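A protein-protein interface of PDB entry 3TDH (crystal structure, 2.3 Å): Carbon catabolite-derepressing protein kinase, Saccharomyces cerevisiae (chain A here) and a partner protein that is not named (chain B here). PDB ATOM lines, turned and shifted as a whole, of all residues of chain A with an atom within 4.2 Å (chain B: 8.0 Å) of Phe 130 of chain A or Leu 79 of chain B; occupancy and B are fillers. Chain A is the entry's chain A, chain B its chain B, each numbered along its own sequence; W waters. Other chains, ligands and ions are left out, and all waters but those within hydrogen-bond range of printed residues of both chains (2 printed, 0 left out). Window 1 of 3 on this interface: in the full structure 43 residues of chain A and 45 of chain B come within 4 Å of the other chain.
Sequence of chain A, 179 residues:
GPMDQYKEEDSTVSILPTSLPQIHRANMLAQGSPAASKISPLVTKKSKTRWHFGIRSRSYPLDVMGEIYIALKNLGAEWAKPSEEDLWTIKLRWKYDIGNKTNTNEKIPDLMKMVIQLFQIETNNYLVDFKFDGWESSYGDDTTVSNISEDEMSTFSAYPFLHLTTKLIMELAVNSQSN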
ATOM      1  N   PHE A  53     -20.795  -1.264  -0.433  1.00  0.00           N
ATOM      2  CA  PHE A  53     -21.843  -2.086  -1.022  1.00  0.00           C
ATOM      3  C   PHE A  53     -21.404  -3.548  -1.000  1.00  0.00           C
ATOM      4  O   PHE A  53     -20.271  -3.864  -1.361  1.00  0.00           O
ATOM      5  CB  PHE A  53     -22.167  -1.632  -2.449  1.00  0.00           C
ATOM      6  CG  PHE A  53     -22.877  -0.310  -2.515  1.00  0.00           C
ATOM      7  CD1 PHE A  53     -24.254  -0.234  -2.317  1.00  0.00           C
ATOM      8  CD2 PHE A  53     -22.171   0.861  -2.763  1.00  0.00           C
ATOM      9  CE1 PHE A  53     -24.912   0.991  -2.369  1.00  0.00           C
ATOM     10  CE2 PHE A  53     -22.823   2.089  -2.818  1.00  0.00           C
ATOM     11  CZ  PHE A  53     -24.191   2.153  -2.619  1.00  0.00           C
ATOM     12  N   GLY A  54     -22.301  -4.423  -0.549  1.00  0.00           N
ATOM     13  CA  GLY A  54     -22.062  -5.865  -0.503  1.00  0.00           C
ATOM     14  C   GLY A  54     -20.834  -6.304   0.277  1.00  0.00           C
ATOM     15  O   GLY A  54     -20.428  -5.653   1.247  1.00  0.00           O
ATOM     16  N   ILE A  55     -20.245  -7.417  -0.151  1.00  0.00           N
ATOM     17  CA  ILE A  55     -19.053  -7.972   0.495  1.00  0.00           C
ATOM     18  C   ILE A  55     -17.944  -8.266  -0.511  1.00  0.00           C
ATOM     19  O   ILE A  55     -18.206  -8.667  -1.647  1.00  0.00           O
ATOM     20  CB  ILE A  55     -19.368  -9.244   1.329  1.00  0.00           C
ATOM     21  CG1 ILE A  55     -20.159 -10.267   0.502  1.00  0.00           C
ATOM     22  CG2 ILE A  55     -20.114  -8.873   2.616  1.00  0.00           C
ATOM     23  CD1 ILE A  55     -20.220 -11.659   1.118  1.00  0.00           C
ATOM     24  N   MET A 114     -34.399 -11.876  -4.995  1.00  0.00           N
ATOM     25  CA  MET A 114     -33.109 -11.199  -4.898  1.00  0.00           C
ATOM     26  C   MET A 114     -32.316 -11.362  -6.188  1.00  0.00           C
ATOM     27  O   MET A 114     -32.453 -12.363  -6.891  1.00  0.00           O
ATOM     28  CB  MET A 114     -32.282 -11.766  -3.742  1.00  0.00           C
ATOM     29  CG  MET A 114     -32.604 -11.209  -2.366  1.00  0.00           C
ATOM     30  SD  MET A 114     -31.491 -11.865  -1.096  1.00  0.00           S
ATOM     31  CE  MET A 114     -29.899 -11.261  -1.653  1.00  0.00           C
ATOM     32  N   VAL A 115     -31.493 -10.366  -6.494  1.00  0.00           N
ATOM     33  CA  VAL A 115     -30.524 -10.466  -7.570  1.00  0.00           C
ATOM     34  C   VAL A 115     -29.126 -10.288  -6.986  1.00  0.00           C
ATOM     35  O   VAL A 115     -28.804  -9.245  -6.407  1.00  0.00           O
ATOM     36  CB  VAL A 115     -30.782  -9.437  -8.704  1.00  0.00           C
ATOM     37  CG1 VAL A 115     -29.699  -9.533  -9.779  1.00  0.00           C
ATOM     38  CG2 VAL A 115     -32.159  -9.648  -9.325  1.00  0.00           C
ATOM     39  N   ILE A 116     -28.311 -11.329  -7.124  1.00  0.00           N
ATOM     40  CA  ILE A 116     -26.922 -11.288  -6.688  1.00  0.00           C
ATOM     41  C   ILE A 116     -26.014 -11.202  -7.910  1.00  0.00           C
ATOM     42  O   ILE A 116     -26.115 -12.015  -8.829  1.00  0.00           O
ATOM     43  CB  ILE A 116     -26.555 -12.506  -5.796  1.00  0.00           C
ATOM     44  CG1 ILE A 116     -27.332 -12.446  -4.474  1.00  0.00           C
ATOM     45  CG2 ILE A 116     -25.046 -12.557  -5.532  1.00  0.00           C
ATOM     46  CD1 ILE A 116     -27.105 -13.638  -3.550  1.00  0.00           C
ATOM     47  N   VAL A 128     -19.328  -8.873  -4.167  1.00  0.00           N
ATOM     48  CA  VAL A 128     -20.628  -9.519  -4.293  1.00  0.00           C
ATOM     49  C   VAL A 128     -21.714  -8.493  -3.962  1.00  0.00           C
ATOM     50  O   VAL A 128     -21.770  -7.976  -2.846  1.00  0.00           O
ATOM     51  CB  VAL A 128     -20.750 -10.743  -3.356  1.00  0.00           C
ATOM     52  CG1 VAL A 128     -22.057 -11.475  -3.602  1.00  0.00           C
ATOM     53  CG2 VAL A 128     -19.570 -11.693  -3.541  1.00  0.00           C
ATOM     54  N   ASP A 129     -22.561  -8.205  -4.948  1.00  0.00           N
ATOM     55  CA  ASP A 129     -23.637  -7.224  -4.819  1.00  0.00           C
ATOM     56  C   ASP A 129     -24.976  -7.923  -4.617  1.00  0.00           C
ATOM     57  O   ASP A 129     -25.306  -8.868  -5.336  1.00  0.00           O
ATOM     58  CB  ASP A 129     -23.678  -6.324  -6.062  1.00  0.00           C
ATOM     59  CG  ASP A 129     -24.914  -5.431  -6.116  1.00  0.00           C
ATOM     60  OD1 ASP A 129     -25.098  -4.581  -5.214  1.00  0.00           O
ATOM     61  OD2 ASP A 129     -25.694  -5.568  -7.081  1.00  0.00           O
ATOM     62  N   PHE A 130     -25.734  -7.452  -3.630  1.00  0.00           N
ATOM     63  CA  PHE A 130     -27.037  -8.020  -3.293  1.00  0.00           C
ATOM     64  C   PHE A 130     -28.123  -6.972  -3.515  1.00  0.00           C
ATOM     65  O   PHE A 130     -28.018  -5.850  -3.024  1.00  0.00           O
ATOM     66  CB  PHE A 130     -27.081  -8.467  -1.826  1.00  0.00           C
ATOM     67  CG  PHE A 130     -25.956  -9.379  -1.419  1.00  0.00           C
ATOM     68  CD1 PHE A 130     -26.148 -10.756  -1.367  1.00  0.00           C
ATOM     69  CD2 PHE A 130     -24.718  -8.862  -1.055  1.00  0.00           C
ATOM     70  CE1 PHE A 130     -25.119 -11.606  -0.981  1.00  0.00           C
ATOM     71  CE2 PHE A 130     -23.682  -9.704  -0.666  1.00  0.00           C
ATOM     72  CZ  PHE A 130     -23.888 -11.082  -0.628  1.00  0.00           C
ATOM     73  N   LYS A 131     -29.170  -7.349  -4.239  1.00  0.00           N
ATOM     74  CA  LYS A 131     -30.260  -6.431  -4.541  1.00  0.00           C
ATOM     75  C   LYS A 131     -31.619  -7.066  -4.275  1.00  0.00           C
ATOM     76  O   LYS A 131     -31.888  -8.184  -4.712  1.00  0.00           O
ATOM     77  CB  LYS A 131     -30.168  -5.954  -5.994  1.00  0.00           C
ATOM     78  CG  LYS A 131     -31.114  -4.817  -6.349  1.00  0.00           C
ATOM     79  CD  LYS A 131     -31.015  -4.462  -7.824  1.00  0.00           C
ATOM     80  CE  LYS A 131     -32.142  -3.536  -8.245  1.00  0.00           C
ATOM     81  NZ  LYS A 131     -33.452  -4.250  -8.266  1.00  0.00           N
ATOM     82  N   PHE A 161     -35.516  -8.089   3.798  1.00  0.00           N
ATOM     83  CA  PHE A 161     -34.379  -8.277   2.900  1.00  0.00           C
ATOM     84  C   PHE A 161     -33.059  -8.185   3.659  1.00  0.00           C
ATOM     85  O   PHE A 161     -32.180  -9.035   3.488  1.00  0.00           O
ATOM     86  CB  PHE A 161     -34.427  -7.252   1.756  1.00  0.00           C
ATOM     87  CG  PHE A 161     -33.135  -7.120   0.986  1.00  0.00           C
ATOM     88  CD1 PHE A 161     -32.750  -8.093   0.062  1.00  0.00           C
ATOM     89  CD2 PHE A 161     -32.315  -6.012   1.168  1.00  0.00           C
ATOM     90  CE1 PHE A 161     -31.558  -7.965  -0.657  1.00  0.00           C
ATOM     91  CE2 PHE A 161     -31.128  -5.878   0.460  1.00  0.00           C
ATOM     92  CZ  PHE A 161     -30.747  -6.857  -0.458  1.00  0.00           C
ATOM     93  N   LEU A 162     -32.932  -7.159   4.500  1.00  0.00           N
ATOM     94  CA  LEU A 162     -31.725  -6.946   5.294  1.00  0.00           C
ATOM     95  C   LEU A 162     -31.465  -8.096   6.268  1.00  0.00           C
ATOM     96  O   LEU A 162     -30.315  -8.496   6.474  1.00  0.00           O
ATOM     97  CB  LEU A 162     -31.794  -5.619   6.055  1.00  0.00           C
ATOM     98  CG  LEU A 162     -31.821  -4.312   5.254  1.00  0.00           C
ATOM     99  CD1 LEU A 162     -31.944  -3.125   6.194  1.00  0.00           C
ATOM    100  CD2 LEU A 162     -30.602  -4.167   4.350  1.00  0.00           C
ATOM    101  N   THR A 165     -30.136 -11.210   4.249  1.00  0.00           N
ATOM    102  CA  THR A 165     -28.749 -11.013   3.825  1.00  0.00           C
ATOM    103  C   THR A 165     -27.780 -11.197   4.994  1.00  0.00           C
ATOM    104  O   THR A 165     -26.666 -11.686   4.804  1.00  0.00           O
ATOM    105  CB  THR A 165     -28.513  -9.640   3.157  1.00  0.00           C
ATOM    106  OG1 THR A 165     -28.958  -8.588   4.022  1.00  0.00           O
ATOM    107  CG2 THR A 165     -29.248  -9.553   1.823  1.00  0.00           C
ATOM    108  N   LEU A 168     -27.224 -14.784   5.190  1.00  0.00           N
ATOM    109  CA  LEU A 168     -26.394 -15.188   4.062  1.00  0.00           C
ATOM    110  C   LEU A 168     -24.918 -14.846   4.273  1.00  0.00           C
ATOM    111  O   LEU A 168     -24.050 -15.684   4.027  1.00  0.00           O
ATOM    112  CB  LEU A 168     -26.929 -14.576   2.761  1.00  0.00           C
ATOM    113  CG  LEU A 168     -26.249 -14.872   1.420  1.00  0.00           C
ATOM    114  CD1 LEU A 168     -25.918 -16.352   1.248  1.00  0.00           C
ATOM    115  CD2 LEU A 168     -27.129 -14.382   0.277  1.00  0.00           C
ATOM    116  N   ILE A 169     -24.647 -13.627   4.738  1.00  0.00           N
ATOM    117  CA  ILE A 169     -23.286 -13.173   5.041  1.00  0.00           C
ATOM    118  C   ILE A 169     -22.636 -14.025   6.141  1.00  0.00           C
ATOM    119  O   ILE A 169     -21.441 -14.332   6.076  1.00  0.00           O
ATOM    120  CB  ILE A 169     -23.261 -11.660   5.413  1.00  0.00           C
ATOM    121  CG1 ILE A 169     -23.613 -10.805   4.188  1.00  0.00           C
ATOM    122  CG2 ILE A 169     -21.902 -11.240   5.973  1.00  0.00           C
ATOM    123  CD1 ILE A 169     -24.004  -9.369   4.515  1.00  0.00           C
ATOM    124  N   LEU B  45     -21.138   2.154  -7.469  1.00  0.00           N
ATOM    125  CA  LEU B  45     -21.042   1.253  -6.320  1.00  0.00           C
ATOM    126  C   LEU B  45     -19.698   1.333  -5.589  1.00  0.00           C
ATOM    127  O   LEU B  45     -19.445   0.557  -4.666  1.00  0.00           O
ATOM    128  CB  LEU B  45     -21.342  -0.194  -6.738  1.00  0.00           C
ATOM    129  CG  LEU B  45     -22.737  -0.539  -7.281  1.00  0.00           C
ATOM    130  CD1 LEU B  45     -22.745  -1.949  -7.847  1.00  0.00           C
ATOM    131  CD2 LEU B  45     -23.822  -0.387  -6.222  1.00  0.00           C
ATOM    132  N   LEU B  50     -20.002   6.291  -1.927  1.00  0.00           N
ATOM    133  CA  LEU B  50     -20.971   5.939  -0.887  1.00  0.00           C
ATOM    134  C   LEU B  50     -20.748   6.695   0.427  1.00  0.00           C
ATOM    135  O   LEU B  50     -21.705   7.176   1.030  1.00  0.00           O
ATOM    136  CB  LEU B  50     -20.976   4.426  -0.641  1.00  0.00           C
ATOM    137  CG  LEU B  50     -21.807   3.851   0.514  1.00  0.00           C
ATOM    138  CD1 LEU B  50     -23.297   4.140   0.359  1.00  0.00           C
ATOM    139  CD2 LEU B  50     -21.563   2.357   0.635  1.00  0.00           C
ATOM    140  N   VAL B  75     -28.111   2.727  -7.086  1.00  0.00           N
ATOM    141  CA  VAL B  75     -27.748   2.046  -5.837  1.00  0.00           C
ATOM    142  C   VAL B  75     -28.935   1.696  -4.932  1.00  0.00           C
ATOM    143  O   VAL B  75     -28.758   1.056  -3.889  1.00  0.00           O
ATOM    144  CB  VAL B  75     -26.675   2.834  -5.027  1.00  0.00           C
ATOM    145  CG1 VAL B  75     -25.469   3.167  -5.904  1.00  0.00           C
ATOM    146  CG2 VAL B  75     -27.266   4.095  -4.392  1.00  0.00           C
ATOM    147  N   LEU B  76     -30.132   2.109  -5.341  1.00  0.00           N
ATOM    148  CA  LEU B  76     -31.346   1.858  -4.571  1.00  0.00           C
ATOM    149  C   LEU B  76     -31.633   0.373  -4.453  1.00  0.00           C
ATOM    150  O   LEU B  76     -31.504  -0.366  -5.429  1.00  0.00           O
ATOM    151  CB  LEU B  76     -32.552   2.574  -5.191  1.00  0.00           C
ATOM    152  CG  LEU B  76     -32.524   4.101  -5.312  1.00  0.00           C
ATOM    153  CD1 LEU B  76     -33.714   4.579  -6.140  1.00  0.00           C
ATOM    154  CD2 LEU B  76     -32.494   4.786  -3.941  1.00  0.00           C
ATOM    155  N   ASN B  77     -32.016  -0.052  -3.248  1.00  0.00           N
ATOM    156  CA  ASN B  77     -32.351  -1.454  -2.953  1.00  0.00           C
ATOM    157  C   ASN B  77     -31.152  -2.416  -2.969  1.00  0.00           C
ATOM    158  O   ASN B  77     -31.323  -3.633  -2.900  1.00  0.00           O
ATOM    159  CB  ASN B  77     -33.490  -1.952  -3.865  1.00  0.00           C
ATOM    160  CG  ASN B  77     -34.711  -1.041  -3.829  1.00  0.00           C
ATOM    161  OD1 ASN B  77     -35.086  -0.531  -2.775  1.00  0.00           O
ATOM    162  ND2 ASN B  77     -35.333  -0.828  -4.986  1.00  0.00           N
ATOM    163  N   HIS B  78     -29.946  -1.860  -3.043  1.00  0.00           N
ATOM    164  CA  HIS B  78     -28.715  -2.639  -2.927  1.00  0.00           C
ATOM    165  C   HIS B  78     -28.239  -2.662  -1.478  1.00  0.00           C
ATOM    166  O   HIS B  78     -28.374  -1.670  -0.756  1.00  0.00           O
ATOM    167  CB  HIS B  78     -27.617  -2.055  -3.820  1.00  0.00           C
ATOM    168  CG  HIS B  78     -27.885  -2.199  -5.286  1.00  0.00           C
ATOM    169  ND1 HIS B  78     -27.181  -3.071  -6.090  1.00  0.00           N
ATOM    170  CD2 HIS B  78     -28.780  -1.583  -6.095  1.00  0.00           C
ATOM    171  CE1 HIS B  78     -27.632  -2.987  -7.329  1.00  0.00           C
ATOM    172  NE2 HIS B  78     -28.601  -2.090  -7.359  1.00  0.00           N
ATOM    173  N   LEU B  79     -27.668  -3.792  -1.067  1.00  0.00           N
ATOM    174  CA  LEU B  79     -27.187  -3.970   0.301  1.00  0.00           C
ATOM    175  C   LEU B  79     -25.928  -3.161   0.584  1.00  0.00           C
ATOM    176  O   LEU B  79     -24.986  -3.156  -0.211  1.00  0.00           O
ATOM    177  CB  LEU B  79     -26.932  -5.454   0.597  1.00  0.00           C
ATOM    178  CG  LEU B  79     -26.403  -5.826   1.989  1.00  0.00           C
ATOM    179  CD1 LEU B  79     -27.475  -5.633   3.048  1.00  0.00           C
ATOM    180  CD2 LEU B  79     -25.893  -7.253   2.006  1.00  0.00           C
ATOM    181  N   VAL B  80     -25.936  -2.474   1.723  1.00  0.00           N
ATOM    182  CA  VAL B  80     -24.763  -1.778   2.243  1.00  0.00           C
ATOM    183  C   VAL B  80     -24.321  -2.488   3.524  1.00  0.00           C
ATOM    184  O   VAL B  80     -25.155  -2.929   4.316  1.00  0.00           O
ATOM    185  CB  VAL B  80     -25.057  -0.281   2.518  1.00  0.00           C
ATOM    186  CG1 VAL B  80     -23.809   0.442   3.005  1.00  0.00           C
ATOM    187  CG2 VAL B  80     -25.592   0.397   1.265  1.00  0.00           C
ATOM    188  N   THR B  81     -23.011  -2.623   3.712  1.00  0.00           N
ATOM    189  CA  THR B  81     -22.464  -3.348   4.855  1.00  0.00           C
ATOM    190  C   THR B  81     -21.337  -2.558   5.502  1.00  0.00           C
ATOM    191  O   THR B  81     -20.814  -1.609   4.915  1.00  0.00           O
ATOM    192  CB  THR B  81     -21.902  -4.751   4.462  1.00  0.00           C
ATOM    193  OG1 THR B  81     -20.685  -4.596   3.724  1.00  0.00           O
ATOM    194  CG2 THR B  81     -22.897  -5.547   3.626  1.00  0.00           C
ATOM    195  N   SER B  82     -20.974  -2.973   6.712  1.00  0.00           N
ATOM    196  CA  SER B  82     -19.817  -2.451   7.426  1.00  0.00           C
ATOM    197  C   SER B  82     -19.133  -3.611   8.144  1.00  0.00           C
ATOM    198  O   SER B  82     -19.683  -4.712   8.211  1.00  0.00           O
ATOM    199  CB  SER B  82     -20.248  -1.379   8.429  1.00  0.00           C
ATOM    200  OG  SER B  82     -21.307  -1.841   9.256  1.00  0.00           O
ATOM    201  N   LEU B  89     -23.766  -7.217  13.505  1.00  0.00           N
ATOM    202  CA  LEU B  89     -23.729  -6.854  12.096  1.00  0.00           C
ATOM    203  C   LEU B  89     -24.643  -5.661  11.842  1.00  0.00           C
ATOM    204  O   LEU B  89     -25.809  -5.651  12.245  1.00  0.00           O
ATOM    205  CB  LEU B  89     -24.098  -8.039  11.196  1.00  0.00           C
ATOM    206  CG  LEU B  89     -23.825  -7.935   9.682  1.00  0.00           C
ATOM    207  CD1 LEU B  89     -22.422  -7.413   9.348  1.00  0.00           C
ATOM    208  CD2 LEU B  89     -24.067  -9.280   9.001  1.00  0.00           C
ATOM    209  N   CYS B  90     -24.087  -4.648  11.194  1.00  0.00           N
ATOM    210  CA  CYS B  90     -24.846  -3.478  10.798  1.00  0.00           C
ATOM    211  C   CYS B  90     -24.928  -3.427   9.281  1.00  0.00           C
ATOM    212  O   CYS B  90     -23.919  -3.240   8.605  1.00  0.00           O
ATOM    213  CB  CYS B  90     -24.199  -2.206  11.349  1.00  0.00           C
ATOM    214  SG  CYS B  90     -25.098  -0.696  10.936  1.00  0.00           S
ATOM    215  N   VAL B  91     -26.134  -3.624   8.757  1.00  0.00           N
ATOM    216  CA  VAL B  91     -26.389  -3.543   7.320  1.00  0.00           C
ATOM    217  C   VAL B  91     -27.410  -2.451   7.011  1.00  0.00           C
ATOM    218  O   VAL B  91     -28.137  -1.998   7.898  1.00  0.00           O
ATOM    219  CB  VAL B  91     -26.869  -4.894   6.723  1.00  0.00           C
ATOM    220  CG1 VAL B  91     -25.738  -5.924   6.736  1.00  0.00           C
ATOM    221  CG2 VAL B  91     -28.122  -5.410   7.444  1.00  0.00           C
ATOM    222  N   ALA B  92     -27.458  -2.032   5.750  1.00  0.00           N
ATOM    223  CA  ALA B  92     -28.342  -0.950   5.333  1.00  0.00           C
ATOM    224  C   ALA B  92     -28.781  -1.104   3.885  1.00  0.00           C
ATOM    225  O   ALA B  92     -28.229  -1.925   3.141  1.00  0.00           O
ATOM    226  CB  ALA B  92     -27.668   0.413   5.550  1.00  0.00           C
ATOM    227  N   SER B  93     -29.789  -0.321   3.505  1.00  0.00           N
ATOM    228  CA  SER B  93     -30.232  -0.211   2.119  1.00  0.00           C
ATOM    229  C   SER B  93     -30.950   1.116   1.897  1.00  0.00           C
ATOM    230  O   SER B  93     -31.830   1.496   2.674  1.00  0.00           O
ATOM    231  CB  SER B  93     -31.148  -1.374   1.737  1.00  0.00           C
ATOM    232  OG  SER B  93     -31.473  -1.315   0.362  1.00  0.00           O
ATOM    233  N   ILE B  94     -30.552   1.816   0.838  1.00  0.00           N
ATOM    234  CA  ILE B  94     -31.170   3.076   0.457  1.00  0.00           C
ATOM    235  C   ILE B  94     -32.410   2.793  -0.389  1.00  0.00           C
ATOM    236  O   ILE B  94     -32.307   2.249  -1.492  1.00  0.00           O
ATOM    237  CB  ILE B  94     -30.182   3.981  -0.315  1.00  0.00           C
ATOM    238  CG1 ILE B  94     -28.858   4.100   0.454  1.00  0.00           C
ATOM    239  CG2 ILE B  94     -30.796   5.363  -0.568  1.00  0.00           C
ATOM    240  CD1 ILE B  94     -27.677   4.561  -0.390  1.00  0.00           C
ATOM    241  N   GLN B 104     -32.283   2.826   5.235  1.00  0.00           N
ATOM    242  CA  GLN B 104     -32.791   1.931   6.278  1.00  0.00           C
ATOM    243  C   GLN B 104     -31.670   1.067   6.859  1.00  0.00           C
ATOM    244  O   GLN B 104     -31.157   0.168   6.196  1.00  0.00           O
ATOM    245  CB  GLN B 104     -33.935   1.057   5.745  1.00  0.00           C
ATOM    246  CG  GLN B 104     -35.213   1.833   5.419  1.00  0.00           C
ATOM    247  CD  GLN B 104     -36.268   1.007   4.701  1.00  0.00           C
ATOM    248  OE1 GLN B 104     -36.014  -0.113   4.264  1.00  0.00           O
ATOM    249  NE2 GLN B 104     -37.460   1.564   4.569  1.00  0.00           N
HETATM  250  O   HOH W   1     -18.775   0.062  -2.114  1.00  0.00           O
HETATM  251  O   HOH W   2     -24.849  -4.908  -2.573  1.00  0.00           O
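Printed residues of chain A that touch a printed residue of chain B: Phe 53, Gly 54, Asp 129, Phe 130, Lys 131, Leu 162, Thr 165 and Ile 169.
Among the printed residues, no Asp or Glu carboxylate lies within 4 Å of a Lys or Arg side-chain nitrogen of the other chain.
Asp 129 of chain A touches just one residue of chain B: His 78.
Printed residues of chain B within 4 Å of Phe 130 of chain A: Asn 77, His 78 and Leu 79.
Of the printed residues of chain B, Ile 169 of chain A touches Leu 79 (3.8 Å).
Of the printed residues of chain A, Leu 45 of chain B touches Phe 53 (3.3 Å).
Of the printed residues of chain A, Val 75 of chain B touches Phe 53 (3.5 Å).
Leu 79 of chain B touches just these residues of chain A: Phe 53, Gly 54, Phe 130, Leu 162, Thr 165 and Ile 169.
Printed residues of chain A within 4 Å of Val 80 of chain B: Phe 53 (3.7 Å).
The nearest printed residue of chain B that does not touch Phe 130 of chain A is Thr 81 of chain B (6.0 Å).
The nearest printed residue of chain A that does not touch Leu 79 of chain B is Phe 161 of chain A (4.2 Å).
The nearest printed residue of chain B that does not touch Lys 131 of chain A is Leu 76 of chain B (4.3 Å).
N of Gly 54 of chain A lies within hydrogen-bond range of O of Leu 79 of chain B, at 3.0 Å.
The backbone carbonyl oxygen (O) of Gly 54 of chain A is in hydrogen-bond range of the side-chain hydroxyl (OG1) of Thr 81 of chain B, 2.7 Å away.
A ring nitrogen (ND1) of His 78 of chain B lies within hydrogen-bond range of the side-chain carboxylate (OD1) of Asp 129 of chain A (2.7 Å).
The backbone carbonyl oxygen (O) of Phe 130 of chain A lies within hydrogen-bond range of the backbone NH (N) of Leu 79 of chain B (2.9 Å).
Water W2 lies within hydrogen-bond range of OD1 of Asp 129 of chain A, N of Phe 130 of chain A, O of Leu 79 of chain B and N of Gly 54 of chain A.
Water W1 lies within hydrogen-bond range of the backbone carbonyl oxygen of Leu 45 of chain B (2.7 Å) and the backbone NH of Phe 53 of chain A (2.9 Å).
N of Val 115 of chain A sits at hydrogen-bond distance from O of Lys 131 of chain A, at 2.8 Å.
The side-chain hydroxyl (OG1) of Thr 165 of chain A is in hydrogen-bond range of the backbone carbonyl oxygen (O) of Phe 161 of chain A, at 3.3 Å.
The backbone carbonyl oxygen (O) of Leu 162 of chain A sits at hydrogen-bond distance from the side-chain hydroxyl (OG1) of Thr 165 of chain A (2.8 Å).
N of Asn 77 of chain B sits at hydrogen-bond distance from O of Ile 94 of chain B (2.9 Å).
The backbone carbonyl oxygen (O) of His 78 of chain B lies within hydrogen-bond range of the side-chain hydroxyl (OG) of Ser 93 of chain B, 3.3 Å away.
N of Val 80 of chain B sits at hydrogen-bond distance from O of Ala 92 of chain B, 2.8 Å away.
Phe 53 of chain A touches Val 75 of chain B.
Phe 53 of chain A touches Val 80 of chain B.
O of Phe 130 of chain A touches O of Asn 77 of chain B (3.98 Å).
CA of His 78 of chain B touches O of Phe 130 of chain A (3.3 Å).
Lys 131 of chain A touches Asn 77 of chain B.
CD of Lys 131 of chain A touches NE2 of His 78 of chain B, 3.4 Å away.
Leu 162 of chain A touches Leu 79 of chain B.
CG2 of Val 91 of chain B touches O of Leu 162 of chain A, at 3.9 Å.
Ala 92 of chain B touches Leu 162 of chain A.
Leu 162 of chain A touches Gln 104 of chain B (CD1 to O, 3.4 Å).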
